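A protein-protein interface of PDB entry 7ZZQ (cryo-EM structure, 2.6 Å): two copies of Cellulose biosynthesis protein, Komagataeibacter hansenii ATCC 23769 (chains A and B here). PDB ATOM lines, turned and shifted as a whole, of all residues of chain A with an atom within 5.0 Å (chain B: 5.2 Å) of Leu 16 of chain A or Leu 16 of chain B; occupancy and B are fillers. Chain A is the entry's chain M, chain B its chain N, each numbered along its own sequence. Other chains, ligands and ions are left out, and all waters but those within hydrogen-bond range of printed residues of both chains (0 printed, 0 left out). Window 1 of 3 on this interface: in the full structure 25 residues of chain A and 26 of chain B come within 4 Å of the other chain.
O of Leu 16 of chain A sits at hydrogen-bond distance from OG of Ser 20 of chain A (2.9 Å).
O of Leu 16 of chain B lies within hydrogen-bond range of OG of Ser 20 of chain B, 2.8 Å away.
CD1 of Phe 12 of chain A touches CD1 of Leu 16 of chain B (3.5 Å).
Phe 12 of chain A touches Val 95 of chain B (CZ to CG1, 3.8 Å).
CD2 of Leu 106 of chain B touches CZ of Phe 15 of chain A, 3.6 Å away.
Leu 16 of chain A touches Phe 12 of chain B (CD1 to CD1, 3.5 Å).
CE2 of Phe 15 of chain B touches CD2 of Leu 16 of chain A, 3.7 Å away.
CD2 of Leu 16 of chain B touches CD2 of Leu 16 of chain A (3.8 Å).
Leu 19 of chain B touches Leu 19 of chain A.
Val 95 of chain A touches Phe 12 of chain B (CG1 to CZ, 3.7 Å).
CD1 of Leu 106 of chain A touches CE1 of Phe 12 of chain B, at 3.9 Å.
Phe 15 of chain B touches Leu 106 of chain A.
Printed residues of chain B within 4 Å of Phe 12 of chain A: Leu 16, Val 95 and Leu 106.
Of chain B, only Phe 12 (3.5 Å), Phe 15 (3.7 Å) and Leu 16 (3.8 Å) come within 4 Å of Leu 16 of chain A.
Ser 20 of chain A touches none of the printed residues of chain B.
Printed residues of chain B within 4 Å of Val 95 of chain A: Phe 12.
Of the printed residues of chain A, Phe 12 of chain B touches Leu 16 (3.5 Å), Val 95 (3.7 Å) and Leu 106 (3.9 Å).
Leu 14 of chain B touches none of the printed residues of chain A.
Printed residues of chain A within 4 Å of Leu 106 of chain B: Phe 12 and Phe 15.
The nearest printed residue of chain B that does not touch Leu 16 of chain A is Leu 19 of chain B (5.2 Å).
The nearest printed residue of chain A that does not touch Leu 16 of chain B is Leu 19 of chain A (5.3 Å).
Of the 12 printed residues of chain B, 6 touch a printed residue of chain A.
Printed residues of chain B that touch a printed residue of chain A: Phe 12, Phe 15, Leu 16, Leu 19, Val 95 and Leu 106.
Hydrophobic or aromatic side chains of chain B within 4 Å of the printed part of chain A: Phe 12, Phe 15, Leu 16, Leu 19, Val 95 and Leu 106.
Among the printed residues, 12 pairs touch across the chains.
Among the printed residues, no Asp or Glu carboxylate lies within 4 Å of a Lys or Arg side-chain nitrogen of the other chain.
Phe 12 of chain A touches Leu 16 of chain B, and with the chains exchanged Leu 16 of chain A touches Phe 12 of chain B.
Phe 12 of chain A touches Leu 106 of chain B, and with the chains exchanged Leu 106 of chain A touches Phe 12 of chain B.
Phe 15 of chain A touches Leu 16 of chain B, and with the chains exchanged Leu 16 of chain A touches Phe 15 of chain B.
Leu 19 of chain A touches its own counterpart, Leu 19 of chain B.
Of the 12 pairs that touch across the chains among the printed residues, 12 have their exchanged pair printed and touching as well.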
ATOM      1  N   PHE A  12     -23.084  21.852  -2.297  1.00  0.00           N
ATOM      2  CA  PHE A  12     -23.614  21.713  -3.646  1.00  0.00           C
ATOM      3  C   PHE A  12     -24.512  22.875  -4.048  1.00  0.00           C
ATOM      4  O   PHE A  12     -25.194  22.789  -5.073  1.00  0.00           O
ATOM      5  CB  PHE A  12     -24.378  20.395  -3.776  1.00  0.00           C
ATOM      6  CG  PHE A  12     -23.534  19.182  -3.520  1.00  0.00           C
ATOM      7  CD1 PHE A  12     -22.514  18.835  -4.388  1.00  0.00           C
ATOM      8  CD2 PHE A  12     -23.763  18.387  -2.410  1.00  0.00           C
ATOM      9  CE1 PHE A  12     -21.738  17.719  -4.154  1.00  0.00           C
ATOM     10  CE2 PHE A  12     -22.990  17.269  -2.171  1.00  0.00           C
ATOM     11  CZ  PHE A  12     -21.976  16.935  -3.044  1.00  0.00           C
ATOM     12  N   THR A  13     -24.531  23.956  -3.267  1.00  0.00           N
ATOM     13  CA  THR A  13     -25.434  25.067  -3.554  1.00  0.00           C
ATOM     14  C   THR A  13     -25.088  25.736  -4.879  1.00  0.00           C
ATOM     15  O   THR A  13     -25.962  25.933  -5.730  1.00  0.00           O
ATOM     16  CB  THR A  13     -25.393  26.083  -2.414  1.00  0.00           C
ATOM     17  OG1 THR A  13     -25.485  25.398  -1.159  1.00  0.00           O
ATOM     18  CG2 THR A  13     -26.550  27.062  -2.536  1.00  0.00           C
ATOM     19  N   LEU A  14     -23.816  26.094  -5.072  1.00  0.00           N
ATOM     20  CA  LEU A  14     -23.403  26.720  -6.325  1.00  0.00           C
ATOM     21  C   LEU A  14     -23.566  25.761  -7.498  1.00  0.00           C
ATOM     22  O   LEU A  14     -23.999  26.161  -8.589  1.00  0.00           O
ATOM     23  CB  LEU A  14     -21.954  27.193  -6.215  1.00  0.00           C
ATOM     24  CG  LEU A  14     -21.422  28.060  -7.356  1.00  0.00           C
ATOM     25  CD1 LEU A  14     -22.175  29.378  -7.425  1.00  0.00           C
ATOM     26  CD2 LEU A  14     -19.932  28.294  -7.197  1.00  0.00           C
ATOM     27  N   PHE A  15     -23.216  24.491  -7.290  1.00  0.00           N
ATOM     28  CA  PHE A  15     -23.410  23.488  -8.329  1.00  0.00           C
ATOM     29  C   PHE A  15     -24.880  23.357  -8.695  1.00  0.00           C
ATOM     30  O   PHE A  15     -25.223  23.244  -9.875  1.00  0.00           O
ATOM     31  CB  PHE A  15     -22.850  22.143  -7.874  1.00  0.00           C
ATOM     32  CG  PHE A  15     -23.290  20.989  -8.726  1.00  0.00           C
ATOM     33  CD1 PHE A  15     -22.711  20.763  -9.962  1.00  0.00           C
ATOM     34  CD2 PHE A  15     -24.290  20.133  -8.294  1.00  0.00           C
ATOM     35  CE1 PHE A  15     -23.118  19.706 -10.749  1.00  0.00           C
ATOM     36  CE2 PHE A  15     -24.702  19.076  -9.079  1.00  0.00           C
ATOM     37  CZ  PHE A  15     -24.116  18.863 -10.308  1.00  0.00           C
ATOM     38  N   LEU A  16     -25.765  23.368  -7.696  1.00  0.00           N
ATOM     39  CA  LEU A  16     -27.191  23.259  -7.982  1.00  0.00           C
ATOM     40  C   LEU A  16     -27.714  24.503  -8.688  1.00  0.00           C
ATOM     41  O   LEU A  16     -28.578  24.402  -9.562  1.00  0.00           O
ATOM     42  CB  LEU A  16     -27.975  22.996  -6.697  1.00  0.00           C
ATOM     43  CG  LEU A  16     -28.052  21.529  -6.272  1.00  0.00           C
ATOM     44  CD1 LEU A  16     -29.100  21.355  -5.198  1.00  0.00           C
ATOM     45  CD2 LEU A  16     -28.352  20.633  -7.463  1.00  0.00           C
ATOM     46  N   GLN A  17     -27.201  25.683  -8.332  1.00  0.00           N
ATOM     47  CA  GLN A  17     -27.585  26.899  -9.043  1.00  0.00           C
ATOM     48  C   GLN A  17     -27.216  26.803 -10.518  1.00  0.00           C
ATOM     49  O   GLN A  17     -28.048  27.050 -11.404  1.00  0.00           O
ATOM     50  CB  GLN A  17     -26.911  28.116  -8.410  1.00  0.00           C
ATOM     51  CG  GLN A  17     -27.362  28.438  -7.001  1.00  0.00           C
ATOM     52  CD  GLN A  17     -26.612  29.614  -6.410  1.00  0.00           C
ATOM     53  OE1 GLN A  17     -26.814  30.759  -6.814  1.00  0.00           O
ATOM     54  NE2 GLN A  17     -25.741  29.338  -5.449  1.00  0.00           N
ATOM     55  N   THR A  18     -25.966  26.424 -10.797  1.00  0.00           N
ATOM     56  CA  THR A  18     -25.521  26.325 -12.183  1.00  0.00           C
ATOM     57  C   THR A  18     -26.276  25.236 -12.936  1.00  0.00           C
ATOM     58  O   THR A  18     -26.643  25.419 -14.102  1.00  0.00           O
ATOM     59  CB  THR A  18     -24.017  26.069 -12.236  1.00  0.00           C
ATOM     60  OG1 THR A  18     -23.347  26.963 -11.343  1.00  0.00           O
ATOM     61  CG2 THR A  18     -23.504  26.296 -13.640  1.00  0.00           C
ATOM     62  N   LEU A  19     -26.517  24.095 -12.286  1.00  0.00           N
ATOM     63  CA  LEU A  19     -27.227  23.003 -12.941  1.00  0.00           C
ATOM     64  C   LEU A  19     -28.675  23.376 -13.230  1.00  0.00           C
ATOM     65  O   LEU A  19     -29.208  23.030 -14.288  1.00  0.00           O
ATOM     66  CB  LEU A  19     -27.154  21.743 -12.078  1.00  0.00           C
ATOM     67  CG  LEU A  19     -28.022  20.563 -12.511  1.00  0.00           C
ATOM     68  CD1 LEU A  19     -27.250  19.643 -13.440  1.00  0.00           C
ATOM     69  CD2 LEU A  19     -28.522  19.806 -11.298  1.00  0.00           C
ATOM     70  N   SER A  20     -29.331  24.074 -12.299  1.00  0.00           N
ATOM     71  CA  SER A  20     -30.692  24.533 -12.544  1.00  0.00           C
ATOM     72  C   SER A  20     -30.735  25.509 -13.709  1.00  0.00           C
ATOM     73  O   SER A  20     -31.615  25.416 -14.572  1.00  0.00           O
ATOM     74  CB  SER A  20     -31.265  25.174 -11.282  1.00  0.00           C
ATOM     75  OG  SER A  20     -30.451  26.241 -10.835  1.00  0.00           O
ATOM     76  N   TRP A  21     -29.779  26.443 -13.760  1.00  0.00           N
ATOM     77  CA  TRP A  21     -29.728  27.369 -14.888  1.00  0.00           C
ATOM     78  C   TRP A  21     -29.522  26.628 -16.204  1.00  0.00           C
ATOM     79  O   TRP A  21     -30.194  26.920 -17.201  1.00  0.00           O
ATOM     80  CB  TRP A  21     -28.616  28.395 -14.671  1.00  0.00           C
ATOM     81  CG  TRP A  21     -29.096  29.699 -14.112  1.00  0.00           C
ATOM     82  CD1 TRP A  21     -29.720  29.898 -12.914  1.00  0.00           C
ATOM     83  CD2 TRP A  21     -28.986  30.987 -14.725  1.00  0.00           C
ATOM     84  NE1 TRP A  21     -30.007  31.230 -12.745  1.00  0.00           N
ATOM     85  CE2 TRP A  21     -29.566  31.920 -13.843  1.00  0.00           C
ATOM     86  CE3 TRP A  21     -28.454  31.442 -15.934  1.00  0.00           C
ATOM     87  CZ2 TRP A  21     -29.629  33.281 -14.133  1.00  0.00           C
ATOM     88  CZ3 TRP A  21     -28.518  32.793 -16.219  1.00  0.00           C
ATOM     89  CH2 TRP A  21     -29.101  33.695 -15.322  1.00  0.00           C
ATOM     90  N   VAL A  95     -32.060  27.245  -4.346  1.00  0.00           N
ATOM     91  CA  VAL A  95     -30.851  27.109  -5.160  1.00  0.00           C
ATOM     92  C   VAL A  95     -30.983  28.067  -6.346  1.00  0.00           C
ATOM     93  O   VAL A  95     -31.559  27.738  -7.387  1.00  0.00           O
ATOM     94  CB  VAL A  95     -30.590  25.661  -5.600  1.00  0.00           C
ATOM     95  CG1 VAL A  95     -30.423  24.784  -4.376  1.00  0.00           C
ATOM     96  CG2 VAL A  95     -31.753  25.083  -6.402  1.00  0.00           C
ATOM     97  N   LEU A 106     -37.031  23.625  -6.679  1.00  0.00           N
ATOM     98  CA  LEU A 106     -37.142  22.261  -6.183  1.00  0.00           C
ATOM     99  C   LEU A 106     -38.555  21.914  -5.726  1.00  0.00           C
ATOM    100  O   LEU A 106     -38.724  21.033  -4.877  1.00  0.00           O
ATOM    101  CB  LEU A 106     -36.150  22.042  -5.040  1.00  0.00           C
ATOM    102  CG  LEU A 106     -34.664  22.075  -5.400  1.00  0.00           C
ATOM    103  CD1 LEU A 106     -33.815  22.110  -4.143  1.00  0.00           C
ATOM    104  CD2 LEU A 106     -34.293  20.883  -6.264  1.00  0.00           C
ATOM    105  N   PHE B  12     -28.117  18.111   0.193  1.00  0.00           N
ATOM    106  CA  PHE B  12     -28.472  17.707  -1.159  1.00  0.00           C
ATOM    107  C   PHE B  12     -27.850  16.378  -1.559  1.00  0.00           C
ATOM    108  O   PHE B  12     -27.905  16.012  -2.735  1.00  0.00           O
ATOM    109  CB  PHE B  12     -28.063  18.792  -2.155  1.00  0.00           C
ATOM    110  CG  PHE B  12     -28.737  20.110  -1.921  1.00  0.00           C
ATOM    111  CD1 PHE B  12     -30.107  20.239  -2.070  1.00  0.00           C
ATOM    112  CD2 PHE B  12     -28.001  21.222  -1.551  1.00  0.00           C
ATOM    113  CE1 PHE B  12     -30.728  21.452  -1.856  1.00  0.00           C
ATOM    114  CE2 PHE B  12     -28.617  22.436  -1.335  1.00  0.00           C
ATOM    115  CZ  PHE B  12     -29.982  22.552  -1.488  1.00  0.00           C
ATOM    116  N   THR B  13     -27.259  15.650  -0.609  1.00  0.00           N
ATOM    117  CA  THR B  13     -26.592  14.396  -0.943  1.00  0.00           C
ATOM    118  C   THR B  13     -27.580  13.375  -1.495  1.00  0.00           C
ATOM    119  O   THR B  13     -27.368  12.815  -2.575  1.00  0.00           O
ATOM    120  CB  THR B  13     -25.876  13.839   0.287  1.00  0.00           C
ATOM    121  OG1 THR B  13     -25.259  14.910   1.010  1.00  0.00           O
ATOM    122  CG2 THR B  13     -24.811  12.840  -0.129  1.00  0.00           C
ATOM    123  N   LEU B  14     -28.672  13.128  -0.770  1.00  0.00           N
ATOM    124  CA  LEU B  14     -29.673  12.175  -1.239  1.00  0.00           C
ATOM    125  C   LEU B  14     -30.346  12.662  -2.515  1.00  0.00           C
ATOM    126  O   LEU B  14     -30.602  11.871  -3.434  1.00  0.00           O
ATOM    127  CB  LEU B  14     -30.710  11.928  -0.145  1.00  0.00           C
ATOM    128  CG  LEU B  14     -31.639  10.735  -0.369  1.00  0.00           C
ATOM    129  CD1 LEU B  14     -31.013   9.463   0.178  1.00  0.00           C
ATOM    130  CD2 LEU B  14     -32.992  10.989   0.268  1.00  0.00           C
ATOM    131  N   PHE B  15     -30.644  13.962  -2.587  1.00  0.00           N
ATOM    132  CA  PHE B  15     -31.229  14.518  -3.799  1.00  0.00           C
ATOM    133  C   PHE B  15     -30.295  14.346  -4.988  1.00  0.00           C
ATOM    134  O   PHE B  15     -30.738  13.995  -6.085  1.00  0.00           O
ATOM    135  CB  PHE B  15     -31.566  15.995  -3.599  1.00  0.00           C
ATOM    136  CG  PHE B  15     -31.817  16.731  -4.882  1.00  0.00           C
ATOM    137  CD1 PHE B  15     -33.001  16.557  -5.575  1.00  0.00           C
ATOM    138  CD2 PHE B  15     -30.863  17.587  -5.404  1.00  0.00           C
ATOM    139  CE1 PHE B  15     -33.231  17.224  -6.759  1.00  0.00           C
ATOM    140  CE2 PHE B  15     -31.089  18.258  -6.588  1.00  0.00           C
ATOM    141  CZ  PHE B  15     -32.275  18.076  -7.266  1.00  0.00           C
ATOM    142  N   LEU B  16     -28.998  14.587  -4.790  1.00  0.00           N
ATOM    143  CA  LEU B  16     -28.048  14.435  -5.888  1.00  0.00           C
ATOM    144  C   LEU B  16     -27.884  12.973  -6.282  1.00  0.00           C
ATOM    145  O   LEU B  16     -27.722  12.663  -7.466  1.00  0.00           O
ATOM    146  CB  LEU B  16     -26.704  15.051  -5.510  1.00  0.00           C
ATOM    147  CG  LEU B  16     -26.575  16.559  -5.732  1.00  0.00           C
ATOM    148  CD1 LEU B  16     -25.118  16.958  -5.825  1.00  0.00           C
ATOM    149  CD2 LEU B  16     -27.329  16.993  -6.981  1.00  0.00           C
ATOM    150  N   GLN B  17     -27.929  12.059  -5.310  1.00  0.00           N
ATOM    151  CA  GLN B  17     -27.883  10.635  -5.628  1.00  0.00           C
ATOM    152  C   GLN B  17     -29.063  10.236  -6.505  1.00  0.00           C
ATOM    153  O   GLN B  17     -28.896   9.584  -7.545  1.00  0.00           O
ATOM    154  CB  GLN B  17     -27.878   9.809  -4.343  1.00  0.00           C
ATOM    155  CG  GLN B  17     -26.622   9.934  -3.507  1.00  0.00           C
ATOM    156  CD  GLN B  17     -26.737   9.209  -2.182  1.00  0.00           C
ATOM    157  OE1 GLN B  17     -26.620   9.814  -1.118  1.00  0.00           O
ATOM    158  NE2 GLN B  17     -26.973   7.905  -2.243  1.00  0.00           N
ATOM    159  N   THR B  18     -30.271  10.634  -6.100  1.00  0.00           N
ATOM    160  CA  THR B  18     -31.456  10.301  -6.881  1.00  0.00           C
ATOM    161  C   THR B  18     -31.428  10.974  -8.248  1.00  0.00           C
ATOM    162  O   THR B  18     -31.841  10.378  -9.248  1.00  0.00           O
ATOM    163  CB  THR B  18     -32.719  10.693  -6.117  1.00  0.00           C
ATOM    164  OG1 THR B  18     -32.594  10.293  -4.748  1.00  0.00           O
ATOM    165  CG2 THR B  18     -33.927  10.015  -6.727  1.00  0.00           C
ATOM    166  N   LEU B  19     -30.954  12.220  -8.309  1.00  0.00           N
ATOM    167  CA  LEU B  19     -30.882  12.929  -9.579  1.00  0.00           C
ATOM    168  C   LEU B  19     -29.900  12.264 -10.531  1.00  0.00           C
ATOM    169  O   LEU B  19     -30.184  12.131 -11.726  1.00  0.00           O
ATOM    170  CB  LEU B  19     -30.495  14.388  -9.340  1.00  0.00           C
ATOM    171  CG  LEU B  19     -30.364  15.279 -10.575  1.00  0.00           C
ATOM    172  CD1 LEU B  19     -31.710  15.860 -10.964  1.00  0.00           C
ATOM    173  CD2 LEU B  19     -29.352  16.381 -10.327  1.00  0.00           C
ATOM    174  N   SER B  20     -28.737  11.847 -10.027  1.00  0.00           N
ATOM    175  CA  SER B  20     -27.780  11.134 -10.863  1.00  0.00           C
ATOM    176  C   SER B  20     -28.360   9.816 -11.357  1.00  0.00           C
ATOM    177  O   SER B  20     -28.225   9.476 -12.537  1.00  0.00           O
ATOM    178  CB  SER B  20     -26.485  10.895 -10.089  1.00  0.00           C
ATOM    179  OG  SER B  20     -26.748  10.373  -8.801  1.00  0.00           O
ATOM    180  N   TRP B  21     -29.019   9.067 -10.466  1.00  0.00           N
ATOM    181  CA  TRP B  21     -29.666   7.824 -10.876  1.00  0.00           C
ATOM    182  C   TRP B  21     -30.674   8.074 -11.993  1.00  0.00           C
ATOM    183  O   TRP B  21     -30.647   7.404 -13.033  1.00  0.00           O
ATOM    184  CB  TRP B  21     -30.352   7.180  -9.670  1.00  0.00           C
ATOM    185  CG  TRP B  21     -30.402   5.685  -9.705  1.00  0.00           C
ATOM    186  CD1 TRP B  21     -31.430   4.911 -10.158  1.00  0.00           C
ATOM    187  CD2 TRP B  21     -29.395   4.780  -9.238  1.00  0.00           C
ATOM    188  NE1 TRP B  21     -31.119   3.581 -10.017  1.00  0.00           N
ATOM    189  CE2 TRP B  21     -29.875   3.474  -9.453  1.00  0.00           C
ATOM    190  CE3 TRP B  21     -28.132   4.949  -8.665  1.00  0.00           C
ATOM    191  CZ2 TRP B  21     -29.137   2.343  -9.116  1.00  0.00           C
ATOM    192  CZ3 TRP B  21     -27.401   3.825  -8.332  1.00  0.00           C
ATOM    193  CH2 TRP B  21     -27.906   2.539  -8.557  1.00  0.00           C
ATOM    194  N   VAL B  95     -21.582  11.345  -4.822  1.00  0.00           N
ATOM    195  CA  VAL B  95     -23.036  11.336  -4.709  1.00  0.00           C
ATOM    196  C   VAL B  95     -23.536  10.011  -5.280  1.00  0.00           C
ATOM    197  O   VAL B  95     -23.864   9.916  -6.469  1.00  0.00           O
ATOM    198  CB  VAL B  95     -23.684  12.536  -5.410  1.00  0.00           C
ATOM    199  CG1 VAL B  95     -23.506  13.779  -4.560  1.00  0.00           C
ATOM    200  CG2 VAL B  95     -23.055  12.775  -6.777  1.00  0.00           C
ATOM    201  N   LEU B 106     -19.645  13.304 -10.573  1.00  0.00           N
ATOM    202  CA  LEU B 106     -19.321  14.715 -10.737  1.00  0.00           C
ATOM    203  C   LEU B 106     -17.969  14.944 -11.400  1.00  0.00           C
ATOM    204  O   LEU B 106     -17.531  16.095 -11.490  1.00  0.00           O
ATOM    205  CB  LEU B 106     -19.351  15.421  -9.378  1.00  0.00           C
ATOM    206  CG  LEU B 106     -20.707  15.513  -8.678  1.00  0.00           C
ATOM    207  CD1 LEU B 106     -20.525  15.838  -7.206  1.00  0.00           C
ATOM    208  CD2 LEU B 106     -21.588  16.548  -9.353  1.00  0.00           C
